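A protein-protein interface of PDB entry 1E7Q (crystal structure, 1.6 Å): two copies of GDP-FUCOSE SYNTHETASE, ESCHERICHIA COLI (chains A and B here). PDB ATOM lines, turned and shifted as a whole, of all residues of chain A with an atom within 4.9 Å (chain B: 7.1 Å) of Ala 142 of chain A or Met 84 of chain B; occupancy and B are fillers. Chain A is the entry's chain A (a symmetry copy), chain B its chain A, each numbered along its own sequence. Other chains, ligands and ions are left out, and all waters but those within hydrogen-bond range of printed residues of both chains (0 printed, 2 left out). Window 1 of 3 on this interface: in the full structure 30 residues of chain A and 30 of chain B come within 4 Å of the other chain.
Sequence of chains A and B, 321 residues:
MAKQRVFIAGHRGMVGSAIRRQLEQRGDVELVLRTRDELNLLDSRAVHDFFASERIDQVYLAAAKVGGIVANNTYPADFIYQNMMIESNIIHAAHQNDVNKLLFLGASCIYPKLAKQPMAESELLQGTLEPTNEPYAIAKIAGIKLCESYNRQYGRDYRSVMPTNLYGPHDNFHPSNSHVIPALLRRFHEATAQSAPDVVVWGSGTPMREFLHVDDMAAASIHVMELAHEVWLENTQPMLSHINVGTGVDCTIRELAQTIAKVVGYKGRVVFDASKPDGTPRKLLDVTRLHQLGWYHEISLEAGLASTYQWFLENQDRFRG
The backbone carbonyl oxygen (O) of Met 84 of chain B sits at hydrogen-bond distance from the side-chain hydroxyl (OG) of Ser 88 of chain B (2.8 Å). The side-chain amide nitrogen of Asn 89 of chain B lies close to the backbone carbonyl oxygen of Met 85 of chain B. OG of Ser 88 of chain A is in hydrogen-bond range of O of Met 84 of chain A.
CE of Met 84 of chain A touches CE of Met 84 of chain B (3.8 Å). OG of Ser 88 of chain B touches CE of Met 84 of chain A, 3.4 Å away. Ala 142 of chain B touches Met 84 of chain A (CB to CE, 3.8 Å). SD of Met 84 of chain A touches CD1 of Leu 146 of chain B (3.8 Å). Ser 88 of chain A touches Tyr 81 of chain B. Ala 142 of chain B touches Ile 138 of chain A (CA to CG2, 3.8 Å). Met 84 of chain B touches Ala 142 of chain A. Ala 142 of chain A touches Ile 138 of chain B. Lys 145 of chain A touches Ile 80 of chain B (CB to CD1, 3.7 Å). Leu 146 of chain A touches Met 84 of chain B (CD1 to SD, 3.8 Å).
Ala 142 of chain A touches three residues of chain B. Met 84 of chain B touches four residues of chain A. Printed residues of chain A within 4 Å of Leu 146 of chain B: Met 84. Of the printed residues of chain A, Tyr 81 of chain B touches Ser 88 (3.7 Å). Of the printed residues of chain B, Met 84 of chain A touches Met 84, Ser 88, Ala 142 and Leu 146. Printed residues of chain A within 4 Å of Ala 142 of chain B: Met 84 and Ile 138. Of the printed residues of chain B, Lys 145 of chain A touches Ile 80 (3.7 Å). Lys 140 of chain A touches none of the printed residues of chain B. The nearest residue of chain B that does not touch Ala 142 of chain A is Ala 142 of chain B (5.0 Å).
Of the 21 printed residues of chain B, 8 touch a printed residue of chain A. Of the 13 printed residues of chain A, 6 touch a printed residue of chain B. Among the printed residues, 14 pairs touch across the chains. Among the printed residues, no Asp or Glu carboxylate lies within 4 Å of a Lys or Arg side-chain nitrogen of the other chain.
Met 84 of chain A touches Ser 88 of chain B, and with the chains exchanged Ser 88 of chain A touches Met 84 of chain B. Met 84 of chain A touches Ala 142 of chain B, and with the chains exchanged Ala 142 of chain A touches Met 84 of chain B. Met 84 of chain A touches Leu 146 of chain B, and with the chains exchanged Leu 146 of chain A touches Met 84 of chain B. Ile 138 of chain A touches Ala 142 of chain B, and with the chains exchanged Ala 142 of chain A touches Ile 138 of chain B. Of the 14 pairs that touch across the chains among the printed residues, 9 have their exchanged pair printed and touching as well.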
ATOM      1  N   MET A  84     -16.024 -33.408 -10.227  1.00  0.00           N
ATOM      2  CA  MET A  84     -14.827 -33.182  -9.382  1.00  0.00           C
ATOM      3  C   MET A  84     -14.495 -34.414  -8.567  1.00  0.00           C
ATOM      4  O   MET A  84     -13.318 -34.778  -8.451  1.00  0.00           O
ATOM      5  CB  MET A  84     -15.017 -31.964  -8.483  1.00  0.00           C
ATOM      6  CG  MET A  84     -15.028 -30.609  -9.158  1.00  0.00           C
ATOM      7  SD  MET A  84     -15.333 -29.237  -8.071  1.00  0.00           S
ATOM      8  CE  MET A  84     -13.914 -29.304  -6.970  1.00  0.00           C
ATOM      9  N   GLU A  87     -13.208 -37.586 -10.660  1.00  0.00           N
ATOM     10  CA  GLU A  87     -11.849 -37.426 -11.149  1.00  0.00           C
ATOM     11  C   GLU A  87     -10.830 -37.365 -10.021  1.00  0.00           C
ATOM     12  O   GLU A  87      -9.759 -38.013 -10.125  1.00  0.00           O
ATOM     13  CB  GLU A  87     -11.856 -36.279 -12.187  1.00  0.00           C
ATOM     14  CG  GLU A  87     -11.886 -34.971 -11.616  1.00  0.00           C
ATOM     15  CD  GLU A  87     -12.499 -34.039 -12.690  1.00  0.00           C
ATOM     16  OE1 GLU A  87     -12.996 -34.128 -13.798  1.00  0.00           O
ATOM     17  OE2 GLU A  87     -12.372 -32.934 -12.211  1.00  0.00           O
ATOM     18  N   SER A  88     -11.170 -36.684  -8.920  1.00  0.00           N
ATOM     19  CA  SER A  88     -10.271 -36.586  -7.766  1.00  0.00           C
ATOM     20  C   SER A  88      -9.984 -37.955  -7.148  1.00  0.00           C
ATOM     21  O   SER A  88      -8.852 -38.360  -6.822  1.00  0.00           O
ATOM     22  CB  SER A  88     -10.925 -35.718  -6.663  1.00  0.00           C
ATOM     23  OG  SER A  88     -10.870 -34.391  -7.143  1.00  0.00           O
ATOM     24  N   ALA A 137     -17.663 -27.642 -17.149  1.00  0.00           N
ATOM     25  CA  ALA A 137     -16.369 -27.321 -17.773  1.00  0.00           C
ATOM     26  C   ALA A 137     -15.318 -27.070 -16.706  1.00  0.00           C
ATOM     27  O   ALA A 137     -14.158 -27.496 -16.877  1.00  0.00           O
ATOM     28  CB  ALA A 137     -16.536 -26.076 -18.644  1.00  0.00           C
ATOM     29  N   ILE A 138     -15.676 -26.332 -15.674  1.00  0.00           N
ATOM     30  CA  ILE A 138     -14.725 -26.132 -14.571  1.00  0.00           C
ATOM     31  C   ILE A 138     -14.283 -27.471 -13.970  1.00  0.00           C
ATOM     32  O   ILE A 138     -13.113 -27.669 -13.683  1.00  0.00           O
ATOM     33  CB  ILE A 138     -15.313 -25.170 -13.527  1.00  0.00           C
ATOM     34  CG1 ILE A 138     -15.498 -23.790 -14.103  1.00  0.00           C
ATOM     35  CG2 ILE A 138     -14.487 -25.172 -12.276  1.00  0.00           C
ATOM     36  CD1 ILE A 138     -14.191 -23.070 -14.338  1.00  0.00           C
ATOM     37  N   ALA A 139     -15.254 -28.374 -13.725  1.00  0.00           N
ATOM     38  CA  ALA A 139     -14.864 -29.692 -13.231  1.00  0.00           C
ATOM     39  C   ALA A 139     -13.900 -30.421 -14.184  1.00  0.00           C
ATOM     40  O   ALA A 139     -12.853 -30.980 -13.757  1.00  0.00           O
ATOM     41  CB  ALA A 139     -16.050 -30.612 -12.980  1.00  0.00           C
ATOM     42  N   LYS A 140     -14.180 -30.349 -15.470  1.00  0.00           N
ATOM     43  CA  LYS A 140     -13.345 -30.993 -16.482  1.00  0.00           C
ATOM     44  C   LYS A 140     -11.945 -30.367 -16.563  1.00  0.00           C
ATOM     45  O   LYS A 140     -10.925 -31.095 -16.620  1.00  0.00           O
ATOM     46  CB  LYS A 140     -14.007 -31.057 -17.852  1.00  0.00           C
ATOM     47  CG  LYS A 140     -15.210 -32.023 -17.929  1.00  0.00           C
ATOM     48  CD  LYS A 140     -14.691 -33.443 -17.787  1.00  0.00           C
ATOM     49  CE  LYS A 140     -15.609 -34.541 -18.247  1.00  0.00           C
ATOM     50  NZ  LYS A 140     -14.937 -35.899 -18.136  1.00  0.00           N
ATOM     51  N   ILE A 141     -11.901 -29.036 -16.500  1.00  0.00           N
ATOM     52  CA  ILE A 141     -10.595 -28.345 -16.486  1.00  0.00           C
ATOM     53  C   ILE A 141      -9.830 -28.710 -15.224  1.00  0.00           C
ATOM     54  O   ILE A 141      -8.619 -29.020 -15.360  1.00  0.00           O
ATOM     55  CB  ILE A 141     -10.755 -26.808 -16.576  1.00  0.00           C
ATOM     56  CG1 ILE A 141     -11.386 -26.461 -17.932  1.00  0.00           C
ATOM     57  CG2 ILE A 141      -9.454 -26.073 -16.328  1.00  0.00           C
ATOM     58  CD1 ILE A 141     -11.883 -25.033 -18.057  1.00  0.00           C
ATOM     59  N   ALA A 142     -10.494 -28.805 -14.076  1.00  0.00           N
ATOM     60  CA  ALA A 142      -9.801 -29.244 -12.862  1.00  0.00           C
ATOM     61  C   ALA A 142      -9.217 -30.663 -13.021  1.00  0.00           C
ATOM     62  O   ALA A 142      -8.156 -30.971 -12.459  1.00  0.00           O
ATOM     63  CB  ALA A 142     -10.732 -29.171 -11.675  1.00  0.00           C
ATOM     64  N   GLY A 143      -9.903 -31.536 -13.825  1.00  0.00           N
ATOM     65  CA  GLY A 143      -9.372 -32.874 -14.052  1.00  0.00           C
ATOM     66  C   GLY A 143      -8.074 -32.792 -14.843  1.00  0.00           C
ATOM     67  O   GLY A 143      -7.159 -33.559 -14.573  1.00  0.00           O
ATOM     68  N   ILE A 144      -8.071 -31.991 -15.902  1.00  0.00           N
ATOM     69  CA  ILE A 144      -6.844 -31.887 -16.697  1.00  0.00           C
ATOM     70  C   ILE A 144      -5.718 -31.366 -15.823  1.00  0.00           C
ATOM     71  O   ILE A 144      -4.596 -31.897 -15.813  1.00  0.00           O
ATOM     72  CB  ILE A 144      -7.080 -30.906 -17.877  1.00  0.00           C
ATOM     73  CG1 ILE A 144      -8.050 -31.469 -18.903  1.00  0.00           C
ATOM     74  CG2 ILE A 144      -5.719 -30.618 -18.492  1.00  0.00           C
ATOM     75  CD1 ILE A 144      -8.532 -30.540 -19.962  1.00  0.00           C
ATOM     76  N   LYS A 145      -6.037 -30.411 -14.947  1.00  0.00           N
ATOM     77  CA  LYS A 145      -4.999 -29.818 -14.073  1.00  0.00           C
ATOM     78  C   LYS A 145      -4.596 -30.732 -12.956  1.00  0.00           C
ATOM     79  O   LYS A 145      -3.445 -30.657 -12.551  1.00  0.00           O
ATOM     80  CB  LYS A 145      -5.457 -28.422 -13.621  1.00  0.00           C
ATOM     81  CG  LYS A 145      -5.730 -27.432 -14.774  1.00  0.00           C
ATOM     82  CD  LYS A 145      -4.501 -27.118 -15.533  1.00  0.00           C
ATOM     83  CE  LYS A 145      -4.676 -26.413 -16.860  1.00  0.00           C
ATOM     84  NZ  LYS A 145      -3.376 -26.158 -17.528  1.00  0.00           N
ATOM     85  N   LEU A 146      -5.470 -31.615 -12.472  1.00  0.00           N
ATOM     86  CA  LEU A 146      -5.040 -32.677 -11.550  1.00  0.00           C
ATOM     87  C   LEU A 146      -4.018 -33.580 -12.293  1.00  0.00           C
ATOM     88  O   LEU A 146      -2.937 -33.821 -11.738  1.00  0.00           O
ATOM     89  CB  LEU A 146      -6.210 -33.596 -11.164  1.00  0.00           C
ATOM     90  CG  LEU A 146      -7.093 -33.039 -10.049  1.00  0.00           C
ATOM     91  CD1 LEU A 146      -8.454 -33.704  -9.983  1.00  0.00           C
ATOM     92  CD2 LEU A 146      -6.361 -33.218  -8.703  1.00  0.00           C
ATOM     93  N   LEU B  42     -10.051 -33.638   4.629  1.00  0.00           N
ATOM     94  CA  LEU B  42      -9.900 -34.394   3.393  1.00  0.00           C
ATOM     95  C   LEU B  42     -10.694 -35.692   3.393  1.00  0.00           C
ATOM     96  O   LEU B  42     -10.946 -36.267   2.346  1.00  0.00           O
ATOM     97  CB  LEU B  42      -8.428 -34.687   3.168  1.00  0.00           C
ATOM     98  CG  LEU B  42      -7.461 -33.566   2.901  1.00  0.00           C
ATOM     99  CD1 LEU B  42      -6.012 -34.031   3.136  1.00  0.00           C
ATOM    100  CD2 LEU B  42      -7.709 -33.039   1.483  1.00  0.00           C
ATOM    101  N   ASP B  78      -0.458 -31.502  -4.591  1.00  0.00           N
ATOM    102  CA  ASP B  78      -1.012 -31.353  -3.232  1.00  0.00           C
ATOM    103  C   ASP B  78      -1.919 -30.090  -3.195  1.00  0.00           C
ATOM    104  O   ASP B  78      -2.994 -30.135  -2.599  1.00  0.00           O
ATOM    105  CB  ASP B  78       0.133 -31.182  -2.244  1.00  0.00           C
ATOM    106  CG  ASP B  78       0.937 -32.483  -2.057  1.00  0.00           C
ATOM    107  OD1 ASP B  78       0.754 -33.497  -2.798  1.00  0.00           O
ATOM    108  OD2 ASP B  78       1.978 -32.261  -1.430  1.00  0.00           O
ATOM    109  N   PHE B  79      -1.503 -29.012  -3.867  1.00  0.00           N
ATOM    110  CA  PHE B  79      -2.315 -27.782  -3.795  1.00  0.00           C
ATOM    111  C   PHE B  79      -3.650 -27.871  -4.555  1.00  0.00           C
ATOM    112  O   PHE B  79      -4.669 -27.377  -4.079  1.00  0.00           O
ATOM    113  CB  PHE B  79      -1.508 -26.586  -4.339  1.00  0.00           C
ATOM    114  CG  PHE B  79      -0.598 -26.035  -3.300  1.00  0.00           C
ATOM    115  CD1 PHE B  79      -1.052 -25.113  -2.378  1.00  0.00           C
ATOM    116  CD2 PHE B  79       0.702 -26.545  -3.196  1.00  0.00           C
ATOM    117  CE1 PHE B  79      -0.217 -24.617  -1.378  1.00  0.00           C
ATOM    118  CE2 PHE B  79       1.521 -26.050  -2.177  1.00  0.00           C
ATOM    119  CZ  PHE B  79       1.102 -25.063  -1.310  1.00  0.00           C
ATOM    120  N   ILE B  80      -3.673 -28.563  -5.721  1.00  0.00           N
ATOM    121  CA  ILE B  80      -4.952 -28.737  -6.393  1.00  0.00           C
ATOM    122  C   ILE B  80      -5.793 -29.802  -5.718  1.00  0.00           C
ATOM    123  O   ILE B  80      -6.974 -29.555  -5.407  1.00  0.00           O
ATOM    124  CB  ILE B  80      -4.826 -28.918  -7.914  1.00  0.00           C
ATOM    125  CG1 ILE B  80      -6.199 -28.997  -8.559  1.00  0.00           C
ATOM    126  CG2 ILE B  80      -4.033 -30.178  -8.264  1.00  0.00           C
ATOM    127  CD1 ILE B  80      -6.186 -28.860 -10.065  1.00  0.00           C
ATOM    128  N   TYR B  81      -5.241 -31.004  -5.442  1.00  0.00           N
ATOM    129  CA  TYR B  81      -6.104 -32.050  -4.869  1.00  0.00           C
ATOM    130  C   TYR B  81      -6.629 -31.693  -3.483  1.00  0.00           C
ATOM    131  O   TYR B  81      -7.820 -31.918  -3.194  1.00  0.00           O
ATOM    132  CB  TYR B  81      -5.299 -33.359  -4.779  1.00  0.00           C
ATOM    133  CG  TYR B  81      -6.044 -34.479  -4.083  1.00  0.00           C
ATOM    134  CD1 TYR B  81      -7.045 -35.164  -4.734  1.00  0.00           C
ATOM    135  CD2 TYR B  81      -5.817 -34.741  -2.756  1.00  0.00           C
ATOM    136  CE1 TYR B  81      -7.805 -36.133  -4.097  1.00  0.00           C
ATOM    137  CE2 TYR B  81      -6.587 -35.677  -2.055  1.00  0.00           C
ATOM    138  CZ  TYR B  81      -7.525 -36.421  -2.770  1.00  0.00           C
ATOM    139  OH  TYR B  81      -8.240 -37.329  -2.056  1.00  0.00           O
ATOM    140  N   GLN B  82      -5.714 -31.222  -2.591  1.00  0.00           N
ATOM    141  CA  GLN B  82      -6.203 -31.004  -1.233  1.00  0.00           C
ATOM    142  C   GLN B  82      -7.300 -29.940  -1.165  1.00  0.00           C
ATOM    143  O   GLN B  82      -8.290 -30.050  -0.443  1.00  0.00           O
ATOM    144  CB  GLN B  82      -5.090 -30.728  -0.218  1.00  0.00           C
ATOM    145  CG  GLN B  82      -4.110 -31.885  -0.107  1.00  0.00           C
ATOM    146  CD  GLN B  82      -2.985 -31.604   0.852  1.00  0.00           C
ATOM    147  OE1 GLN B  82      -3.136 -30.782   1.769  1.00  0.00           O
ATOM    148  NE2 GLN B  82      -1.877 -32.290   0.586  1.00  0.00           N
ATOM    149  N   ASN B  83      -7.128 -28.854  -1.938  1.00  0.00           N
ATOM    150  CA  ASN B  83      -8.114 -27.772  -1.904  1.00  0.00           C
ATOM    151  C   ASN B  83      -9.395 -28.202  -2.622  1.00  0.00           C
ATOM    152  O   ASN B  83     -10.474 -27.943  -2.066  1.00  0.00           O
ATOM    153  CB  ASN B  83      -7.501 -26.514  -2.468  1.00  0.00           C
ATOM    154  CG  ASN B  83      -6.509 -25.917  -1.452  1.00  0.00           C
ATOM    155  OD1 ASN B  83      -6.906 -25.665  -0.287  1.00  0.00           O
ATOM    156  ND2 ASN B  83      -5.266 -25.787  -1.905  1.00  0.00           N
ATOM    157  N   MET B  84      -9.281 -28.990  -3.691  1.00  0.00           N
ATOM    158  CA  MET B  84     -10.540 -29.523  -4.265  1.00  0.00           C
ATOM    159  C   MET B  84     -11.288 -30.361  -3.251  1.00  0.00           C
ATOM    160  O   MET B  84     -12.517 -30.250  -3.144  1.00  0.00           O
ATOM    161  CB  MET B  84     -10.265 -30.318  -5.538  1.00  0.00           C
ATOM    162  CG  MET B  84      -9.824 -29.532  -6.754  1.00  0.00           C
ATOM    163  SD  MET B  84      -9.441 -30.519  -8.181  1.00  0.00           S
ATOM    164  CE  MET B  84     -11.026 -31.281  -8.550  1.00  0.00           C
ATOM    165  N   MET B  85     -10.585 -31.305  -2.577  1.00  0.00           N
ATOM    166  CA  MET B  85     -11.289 -32.229  -1.667  1.00  0.00           C
ATOM    167  C   MET B  85     -11.863 -31.477  -0.469  1.00  0.00           C
ATOM    168  O   MET B  85     -12.967 -31.770   0.008  1.00  0.00           O
ATOM    169  CB  MET B  85     -10.331 -33.373  -1.183  1.00  0.00           C
ATOM    170  CG  MET B  85      -9.948 -34.353  -2.226  1.00  0.00           C
ATOM    171  SD  MET B  85     -11.389 -35.183  -3.011  1.00  0.00           S
ATOM    172  CE  MET B  85     -12.340 -35.434  -1.591  1.00  0.00           C
ATOM    173  N   ILE B  86     -11.095 -30.597   0.172  1.00  0.00           N
ATOM    174  CA  ILE B  86     -11.578 -29.886   1.366  1.00  0.00           C
ATOM    175  C   ILE B  86     -12.849 -29.131   0.977  1.00  0.00           C
ATOM    176  O   ILE B  86     -13.860 -29.195   1.689  1.00  0.00           O
ATOM    177  CB  ILE B  86     -10.515 -28.897   1.864  1.00  0.00           C
ATOM    178  CG1 ILE B  86      -9.344 -29.675   2.508  1.00  0.00           C
ATOM    179  CG2 ILE B  86     -11.118 -27.920   2.859  1.00  0.00           C
ATOM    180  CD1 ILE B  86      -8.115 -28.801   2.760  1.00  0.00           C
ATOM    181  N   GLU B  87     -12.810 -28.358  -0.125  1.00  0.00           N
ATOM    182  CA  GLU B  87     -13.979 -27.568  -0.476  1.00  0.00           C
ATOM    183  C   GLU B  87     -15.159 -28.430  -0.895  1.00  0.00           C
ATOM    184  O   GLU B  87     -16.305 -28.157  -0.461  1.00  0.00           O
ATOM    185  CB  GLU B  87     -13.516 -26.449  -1.440  1.00  0.00           C
ATOM    186  CG  GLU B  87     -13.309 -26.881  -2.785  1.00  0.00           C
ATOM    187  CD  GLU B  87     -12.308 -25.883  -3.416  1.00  0.00           C
ATOM    188  OE1 GLU B  87     -11.636 -24.926  -3.075  1.00  0.00           O
ATOM    189  OE2 GLU B  87     -12.278 -26.211  -4.582  1.00  0.00           O
ATOM    190  N   SER B  88     -14.899 -29.507  -1.647  1.00  0.00           N
ATOM    191  CA  SER B  88     -15.961 -30.419  -2.082  1.00  0.00           C
ATOM    192  C   SER B  88     -16.658 -31.089  -0.897  1.00  0.00           C
ATOM    193  O   SER B  88     -17.894 -31.195  -0.772  1.00  0.00           O
ATOM    194  CB  SER B  88     -15.360 -31.548  -2.954  1.00  0.00           C
ATOM    195  OG  SER B  88     -15.025 -30.940  -4.184  1.00  0.00           O
ATOM    196  N   ASN B  89     -15.845 -31.565   0.033  1.00  0.00           N
ATOM    197  CA  ASN B  89     -16.348 -32.260   1.206  1.00  0.00           C
ATOM    198  C   ASN B  89     -17.197 -31.326   2.049  1.00  0.00           C
ATOM    199  O   ASN B  89     -18.316 -31.711   2.472  1.00  0.00           O
ATOM    200  CB  ASN B  89     -15.192 -32.792   2.037  1.00  0.00           C
ATOM    201  CG  ASN B  89     -14.514 -33.997   1.408  1.00  0.00           C
ATOM    202  OD1 ASN B  89     -15.040 -34.689   0.527  1.00  0.00           O
ATOM    203  ND2 ASN B  89     -13.351 -34.333   1.987  1.00  0.00           N
ATOM    204  N   ILE B  90     -16.629 -30.121   2.379  1.00  0.00           N
ATOM    205  CA  ILE B  90     -17.427 -29.241   3.229  1.00  0.00           C
ATOM    206  C   ILE B  90     -18.700 -28.738   2.586  1.00  0.00           C
ATOM    207  O   ILE B  90     -19.791 -28.754   3.191  1.00  0.00           O
ATOM    208  CB  ILE B  90     -16.562 -28.075   3.747  1.00  0.00           C
ATOM    209  CG1 ILE B  90     -15.464 -28.589   4.649  1.00  0.00           C
ATOM    210  CG2 ILE B  90     -17.424 -27.001   4.385  1.00  0.00           C
ATOM    211  CD1 ILE B  90     -14.404 -27.533   4.958  1.00  0.00           C
ATOM    212  N   PRO B 135      -2.417 -24.459 -10.284  1.00  0.00           N
ATOM    213  CA  PRO B 135      -3.093 -25.575  -9.652  1.00  0.00           C
ATOM    214  C   PRO B 135      -4.011 -25.096  -8.516  1.00  0.00           C
ATOM    215  O   PRO B 135      -5.193 -25.450  -8.356  1.00  0.00           O
ATOM    216  CB  PRO B 135      -1.989 -26.566  -9.225  1.00  0.00           C
ATOM    217  CG  PRO B 135      -0.881 -26.207 -10.222  1.00  0.00           C
ATOM    218  CD  PRO B 135      -0.982 -24.713 -10.439  1.00  0.00           C
ATOM    219  N   ILE B 138      -6.987 -22.933  -9.848  1.00  0.00           N
ATOM    220  CA  ILE B 138      -8.067 -23.774 -10.386  1.00  0.00           C
ATOM    221  C   ILE B 138      -8.902 -24.391  -9.258  1.00  0.00           C
ATOM    222  O   ILE B 138     -10.120 -24.430  -9.336  1.00  0.00           O
ATOM    223  CB  ILE B 138      -7.496 -24.822 -11.353  1.00  0.00           C
ATOM    224  CG1 ILE B 138      -6.901 -24.168 -12.574  1.00  0.00           C
ATOM    225  CG2 ILE B 138      -8.530 -25.854 -11.691  1.00  0.00           C
ATOM    226  CD1 ILE B 138      -7.946 -23.581 -13.494  1.00  0.00           C
ATOM    227  N   ALA B 139      -8.221 -24.931  -8.227  1.00  0.00           N
ATOM    228  CA  ALA B 139      -8.982 -25.454  -7.095  1.00  0.00           C
ATOM    229  C   ALA B 139      -9.878 -24.388  -6.441  1.00  0.00           C
ATOM    230  O   ALA B 139     -11.086 -24.626  -6.163  1.00  0.00           O
ATOM    231  CB  ALA B 139      -8.102 -26.050  -6.007  1.00  0.00           C
ATOM    232  N   LYS B 140      -9.343 -23.195  -6.272  1.00  0.00           N
ATOM    233  CA  LYS B 140     -10.087 -22.092  -5.666  1.00  0.00           C
ATOM    234  C   LYS B 140     -11.270 -21.642  -6.535  1.00  0.00           C
ATOM    235  O   LYS B 140     -12.395 -21.433  -6.020  1.00  0.00           O
ATOM    236  CB  LYS B 140      -9.200 -20.915  -5.279  1.00  0.00           C
ATOM    237  CG  LYS B 140      -8.249 -21.201  -4.095  1.00  0.00           C
ATOM    238  CD  LYS B 140      -9.086 -21.364  -2.839  1.00  0.00           C
ATOM    239  CE  LYS B 140      -8.363 -21.228  -1.530  1.00  0.00           C
ATOM    240  NZ  LYS B 140      -9.326 -21.320  -0.358  1.00  0.00           N
ATOM    241  N   ALA B 142     -12.796 -23.581  -8.688  1.00  0.00           N
ATOM    242  CA  ALA B 142     -13.793 -24.650  -8.571  1.00  0.00           C
ATOM    243  C   ALA B 142     -14.633 -24.506  -7.286  1.00  0.00           C
ATOM    244  O   ALA B 142     -15.825 -24.846  -7.273  1.00  0.00           O
ATOM    245  CB  ALA B 142     -13.119 -26.000  -8.629  1.00  0.00           C
ATOM    246  N   GLY B 143     -14.014 -23.963  -6.190  1.00  0.00           N
ATOM    247  CA  GLY B 143     -14.772 -23.756  -4.963  1.00  0.00           C
ATOM    248  C   GLY B 143     -15.841 -22.694  -5.183  1.00  0.00           C
ATOM    249  O   GLY B 143     -16.937 -22.829  -4.656  1.00  0.00           O
ATOM    250  N   LEU B 146     -18.532 -24.303  -7.172  1.00  0.00           N
ATOM    251  CA  LEU B 146     -19.357 -25.208  -6.357  1.00  0.00           C
ATOM    252  C   LEU B 146     -20.389 -24.349  -5.574  1.00  0.00           C
ATOM    253  O   LEU B 146     -21.583 -24.673  -5.630  1.00  0.00           O
ATOM    254  CB  LEU B 146     -18.518 -25.931  -5.291  1.00  0.00           C
ATOM    255  CG  LEU B 146     -17.768 -27.153  -5.818  1.00  0.00           C
ATOM    256  CD1 LEU B 146     -16.627 -27.583  -4.917  1.00  0.00           C
ATOM    257  CD2 LEU B 146     -18.770 -28.315  -5.980  1.00  0.00           C
